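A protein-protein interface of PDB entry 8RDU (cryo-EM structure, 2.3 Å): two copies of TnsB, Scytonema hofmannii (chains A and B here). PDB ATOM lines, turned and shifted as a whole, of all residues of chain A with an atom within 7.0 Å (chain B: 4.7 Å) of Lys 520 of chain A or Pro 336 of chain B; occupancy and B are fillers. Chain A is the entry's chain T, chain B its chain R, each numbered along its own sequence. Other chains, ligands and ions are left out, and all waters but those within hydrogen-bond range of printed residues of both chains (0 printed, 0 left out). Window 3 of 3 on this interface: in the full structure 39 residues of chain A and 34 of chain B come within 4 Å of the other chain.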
ATOM      1  N   ASP A 514     -29.202 -24.203 -23.283  1.00  0.00           N
ATOM      2  CA  ASP A 514     -29.404 -23.576 -24.588  1.00  0.00           C
ATOM      3  C   ASP A 514     -29.934 -22.148 -24.486  1.00  0.00           C
ATOM      4  O   ASP A 514     -29.485 -21.265 -25.223  1.00  0.00           O
ATOM      5  CB  ASP A 514     -30.322 -24.440 -25.442  1.00  0.00           C
ATOM      6  CG  ASP A 514     -29.647 -25.715 -25.898  1.00  0.00           C
ATOM      7  OD1 ASP A 514     -28.437 -25.868 -25.629  1.00  0.00           O
ATOM      8  OD2 ASP A 514     -30.321 -26.554 -26.529  1.00  0.00           O
ATOM      9  N   ALA A 515     -30.871 -21.894 -23.571  1.00  0.00           N
ATOM     10  CA  ALA A 515     -31.355 -20.532 -23.369  1.00  0.00           C
ATOM     11  C   ALA A 515     -30.250 -19.579 -22.933  1.00  0.00           C
ATOM     12  O   ALA A 515     -30.295 -18.390 -23.263  1.00  0.00           O
ATOM     13  CB  ALA A 515     -32.490 -20.527 -22.344  1.00  0.00           C
ATOM     14  N   LEU A 516     -29.251 -20.072 -22.206  1.00  0.00           N
ATOM     15  CA  LEU A 516     -28.053 -19.275 -21.966  1.00  0.00           C
ATOM     16  C   LEU A 516     -27.258 -19.089 -23.250  1.00  0.00           C
ATOM     17  O   LEU A 516     -26.974 -17.959 -23.660  1.00  0.00           O
ATOM     18  CB  LEU A 516     -27.198 -19.927 -20.874  1.00  0.00           C
ATOM     19  CG  LEU A 516     -25.895 -19.265 -20.394  1.00  0.00           C
ATOM     20  CD1 LEU A 516     -24.724 -19.370 -21.368  1.00  0.00           C
ATOM     21  CD2 LEU A 516     -26.170 -17.811 -20.055  1.00  0.00           C
ATOM     22  N   VAL A 517     -26.883 -20.193 -23.897  1.00  0.00           N
ATOM     23  CA  VAL A 517     -26.053 -20.119 -25.096  1.00  0.00           C
ATOM     24  C   VAL A 517     -26.731 -19.321 -26.204  1.00  0.00           C
ATOM     25  O   VAL A 517     -26.055 -18.718 -27.048  1.00  0.00           O
ATOM     26  CB  VAL A 517     -25.695 -21.546 -25.553  1.00  0.00           C
ATOM     27  CG1 VAL A 517     -25.164 -21.547 -26.956  1.00  0.00           C
ATOM     28  CG2 VAL A 517     -24.667 -22.136 -24.624  1.00  0.00           C
ATOM     29  N   ALA A 518     -28.064 -19.262 -26.201  1.00  0.00           N
ATOM     30  CA  ALA A 518     -28.774 -18.414 -27.154  1.00  0.00           C
ATOM     31  C   ALA A 518     -28.358 -16.949 -27.084  1.00  0.00           C
ATOM     32  O   ALA A 518     -28.576 -16.211 -28.050  1.00  0.00           O
ATOM     33  CB  ALA A 518     -30.280 -18.528 -26.927  1.00  0.00           C
ATOM     34  N   THR A 519     -27.760 -16.507 -25.980  1.00  0.00           N
ATOM     35  CA  THR A 519     -27.259 -15.142 -25.893  1.00  0.00           C
ATOM     36  C   THR A 519     -25.897 -14.950 -26.546  1.00  0.00           C
ATOM     37  O   THR A 519     -25.476 -13.804 -26.730  1.00  0.00           O
ATOM     38  CB  THR A 519     -27.202 -14.699 -24.435  1.00  0.00           C
ATOM     39  OG1 THR A 519     -26.210 -15.463 -23.742  1.00  0.00           O
ATOM     40  CG2 THR A 519     -28.553 -14.895 -23.775  1.00  0.00           C
ATOM     41  N   LYS A 520     -25.203 -16.028 -26.898  1.00  0.00           N
ATOM     42  CA  LYS A 520     -23.881 -15.915 -27.502  1.00  0.00           C
ATOM     43  C   LYS A 520     -23.948 -15.257 -28.874  1.00  0.00           C
ATOM     44  O   LYS A 520     -24.757 -15.642 -29.723  1.00  0.00           O
ATOM     45  CB  LYS A 520     -23.261 -17.305 -27.622  1.00  0.00           C
ATOM     46  CG  LYS A 520     -21.883 -17.359 -28.237  1.00  0.00           C
ATOM     47  CD  LYS A 520     -21.950 -17.774 -29.702  1.00  0.00           C
ATOM     48  CE  LYS A 520     -20.613 -17.595 -30.390  1.00  0.00           C
ATOM     49  NZ  LYS A 520     -20.688 -17.904 -31.836  1.00  0.00           N
ATOM     50  N   LYS A 521     -23.078 -14.270 -29.096  1.00  0.00           N
ATOM     51  CA  LYS A 521     -22.688 -13.843 -30.431  1.00  0.00           C
ATOM     52  C   LYS A 521     -21.186 -13.613 -30.444  1.00  0.00           C
ATOM     53  O   LYS A 521     -20.634 -13.050 -29.497  1.00  0.00           O
ATOM     54  CB  LYS A 521     -23.415 -12.566 -30.855  1.00  0.00           C
ATOM     55  CG  LYS A 521     -23.137 -12.159 -32.290  1.00  0.00           C
ATOM     56  CD  LYS A 521     -23.573 -10.729 -32.573  1.00  0.00           C
ATOM     57  CE  LYS A 521     -22.991 -10.221 -33.886  1.00  0.00           C
ATOM     58  NZ  LYS A 521     -21.540  -9.900 -33.773  1.00  0.00           N
ATOM     59  N   SER A 522     -20.529 -14.038 -31.517  1.00  0.00           N
ATOM     60  CA  SER A 522     -19.118 -13.719 -31.713  1.00  0.00           C
ATOM     61  C   SER A 522     -18.885 -12.249 -32.041  1.00  0.00           C
ATOM     62  O   SER A 522     -17.980 -11.614 -31.496  1.00  0.00           O
ATOM     63  CB  SER A 522     -18.522 -14.597 -32.810  1.00  0.00           C
ATOM     64  OG  SER A 522     -18.494 -15.952 -32.408  1.00  0.00           O
ATOM     65  N   VAL B 211     -12.934 -26.243 -24.826  1.00  0.00           N
ATOM     66  CA  VAL B 211     -13.597 -25.008 -25.212  1.00  0.00           C
ATOM     67  C   VAL B 211     -12.552 -23.908 -25.188  1.00  0.00           C
ATOM     68  O   VAL B 211     -11.846 -23.739 -24.189  1.00  0.00           O
ATOM     69  CB  VAL B 211     -14.774 -24.674 -24.280  1.00  0.00           C
ATOM     70  CG1 VAL B 211     -15.264 -23.273 -24.534  1.00  0.00           C
ATOM     71  CG2 VAL B 211     -15.895 -25.659 -24.497  1.00  0.00           C
ATOM     72  N   THR B 334     -21.435 -29.553 -26.813  1.00  0.00           N
ATOM     73  CA  THR B 334     -22.659 -28.843 -27.155  1.00  0.00           C
ATOM     74  C   THR B 334     -22.562 -27.343 -26.909  1.00  0.00           C
ATOM     75  O   THR B 334     -23.593 -26.669 -26.836  1.00  0.00           O
ATOM     76  CB  THR B 334     -23.859 -29.421 -26.403  1.00  0.00           C
ATOM     77  OG1 THR B 334     -25.054 -28.818 -26.906  1.00  0.00           O
ATOM     78  CG2 THR B 334     -23.782 -29.134 -24.923  1.00  0.00           C
ATOM     79  N   LEU B 335     -21.350 -26.808 -26.780  1.00  0.00           N
ATOM     80  CA  LEU B 335     -21.161 -25.413 -26.422  1.00  0.00           C
ATOM     81  C   LEU B 335     -20.426 -24.652 -27.516  1.00  0.00           C
ATOM     82  O   LEU B 335     -19.573 -25.212 -28.209  1.00  0.00           O
ATOM     83  CB  LEU B 335     -20.379 -25.273 -25.111  1.00  0.00           C
ATOM     84  CG  LEU B 335     -21.082 -25.784 -23.862  1.00  0.00           C
ATOM     85  CD1 LEU B 335     -20.188 -25.623 -22.649  1.00  0.00           C
ATOM     86  CD2 LEU B 335     -22.404 -25.063 -23.670  1.00  0.00           C
ATOM     87  N   PRO B 336     -20.739 -23.367 -27.678  1.00  0.00           N
ATOM     88  CA  PRO B 336     -20.018 -22.528 -28.639  1.00  0.00           C
ATOM     89  C   PRO B 336     -18.513 -22.567 -28.444  1.00  0.00           C
ATOM     90  O   PRO B 336     -17.997 -22.284 -27.366  1.00  0.00           O
ATOM     91  CB  PRO B 336     -20.571 -21.128 -28.357  1.00  0.00           C
ATOM     92  CG  PRO B 336     -21.888 -21.358 -27.765  1.00  0.00           C
ATOM     93  CD  PRO B 336     -21.766 -22.602 -26.955  1.00  0.00           C
ATOM     94  N   GLY B 337     -17.807 -22.881 -29.515  1.00  0.00           N
ATOM     95  CA  GLY B 337     -16.366 -22.929 -29.478  1.00  0.00           C
ATOM     96  C   GLY B 337     -15.775 -24.231 -29.016  1.00  0.00           C
ATOM     97  O   GLY B 337     -14.610 -24.254 -28.609  1.00  0.00           O
ATOM     98  N   TYR B 338     -16.537 -25.316 -29.059  1.00  0.00           N
ATOM     99  CA  TYR B 338     -15.965 -26.640 -28.885  1.00  0.00           C
ATOM    100  C   TYR B 338     -14.811 -26.840 -29.851  1.00  0.00           C
ATOM    101  O   TYR B 338     -14.946 -26.611 -31.052  1.00  0.00           O
ATOM    102  CB  TYR B 338     -17.034 -27.704 -29.108  1.00  0.00           C
ATOM    103  CG  TYR B 338     -16.515 -29.114 -29.016  1.00  0.00           C
ATOM    104  CD1 TYR B 338     -15.972 -29.603 -27.845  1.00  0.00           C
ATOM    105  CD2 TYR B 338     -16.550 -29.949 -30.114  1.00  0.00           C
ATOM    106  CE1 TYR B 338     -15.512 -30.895 -27.766  1.00  0.00           C
ATOM    107  CE2 TYR B 338     -16.077 -31.228 -30.049  1.00  0.00           C
ATOM    108  CZ  TYR B 338     -15.562 -31.700 -28.877  1.00  0.00           C
ATOM    109  OH  TYR B 338     -15.071 -32.980 -28.822  1.00  0.00           O
ATOM    110  N   ASP B 353     -15.904 -19.267 -33.662  1.00  0.00           N
ATOM    111  CA  ASP B 353     -17.101 -19.464 -32.851  1.00  0.00           C
ATOM    112  C   ASP B 353     -16.871 -19.232 -31.365  1.00  0.00           C
ATOM    113  O   ASP B 353     -17.844 -19.068 -30.623  1.00  0.00           O
ATOM    114  CB  ASP B 353     -17.691 -20.851 -33.070  1.00  0.00           C
ATOM    115  CG  ASP B 353     -19.149 -20.913 -32.667  1.00  0.00           C
ATOM    116  OD1 ASP B 353     -19.791 -19.842 -32.644  1.00  0.00           O
ATOM    117  OD2 ASP B 353     -19.658 -22.017 -32.386  1.00  0.00           O
ATOM    118  N   ARG B 355     -16.969 -18.193 -28.027  1.00  0.00           N
ATOM    119  CA  ARG B 355     -17.547 -17.229 -27.090  1.00  0.00           C
ATOM    120  C   ARG B 355     -18.186 -18.022 -25.946  1.00  0.00           C
ATOM    121  O   ARG B 355     -19.339 -18.439 -26.039  1.00  0.00           O
ATOM    122  CB  ARG B 355     -18.549 -16.312 -27.772  1.00  0.00           C
ATOM    123  CG  ARG B 355     -19.142 -15.151 -26.925  1.00  0.00           C
ATOM    124  CD  ARG B 355     -20.077 -15.655 -25.814  1.00  0.00           C
ATOM    125  NE  ARG B 355     -20.740 -14.646 -25.002  1.00  0.00           N
ATOM    126  CZ  ARG B 355     -21.380 -14.915 -23.872  1.00  0.00           C
ATOM    127  NH1 ARG B 355     -21.768 -16.143 -23.578  1.00  0.00           N
ATOM    128  NH2 ARG B 355     -21.743 -13.915 -23.078  1.00  0.00           N
ATOM    129  N   LEU B 356     -17.393 -18.267 -24.906  1.00  0.00           N
ATOM    130  CA  LEU B 356     -17.845 -18.424 -23.533  1.00  0.00           C
ATOM    131  C   LEU B 356     -16.716 -17.915 -22.654  1.00  0.00           C
ATOM    132  O   LEU B 356     -15.544 -18.057 -23.003  1.00  0.00           O
ATOM    133  CB  LEU B 356     -18.212 -19.869 -23.179  1.00  0.00           C
ATOM    134  CG  LEU B 356     -19.505 -20.459 -23.743  1.00  0.00           C
ATOM    135  CD1 LEU B 356     -19.724 -21.869 -23.253  1.00  0.00           C
ATOM    136  CD2 LEU B 356     -20.670 -19.584 -23.340  1.00  0.00           C
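Val 517 of chain A touches Leu 335 of chain B (CG2 to CD2, 3.8 Å).
Val 517 of chain A touches Pro 336 of chain B.
Lys 520 of chain A touches Pro 336 of chain B.
Lys 520 of chain A touches Arg 355 of chain B (CG to CD, 3.5 Å).
Arg 355 of chain B touches Lys 521 of chain A.
O of Asp 353 of chain B touches OG of Ser 522 of chain A (3.6 Å).
NZ of Lys 520 of chain A sits at hydrogen-bond distance from OG of Ser 522 of chain A (3.0 Å).
No position is printed for both chains.
Hydrophobic or aromatic side chains of chain A within 4 Å of the printed part of chain B: Val 517.
Of the 9 printed residues of chain B, 4 touch a printed residue of chain A.
Hydrophobic or aromatic side chains of chain B that line the printed part of chain A: Leu 335 and Pro 336.
Among the printed residues, Asp or Glu carboxylates within 4 Å of a Lys or Arg side-chain nitrogen of the other chain: Lys 520 of chain A with Asp 353 of chain B.
Asp 514 of chain A touches none of the printed residues of chain B.
Of the printed residues of chain B, Val 517 of chain A touches Leu 335 and Pro 336.
Of the printed residues of chain B, Lys 521 of chain A touches Arg 355.
Pro 336 of chain B touches just these residues of chain A: Val 517 and Lys 520.
Of the printed residues of chain A, Asp 353 of chain B touches Lys 520 (2.3 Å) and Ser 522 (3.6 Å).
Of the printed residues of chain A, Arg 355 of chain B touches Lys 520 (3.5 Å) and Lys 521 (3.6 Å).
The nearest residue of chain A that does not touch Pro 336 of chain B is Ala 518 of chain A (6.7 Å).
O of Asp 353 of chain B lies close to NZ of Lys 520 of chain A (3.3 Å).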
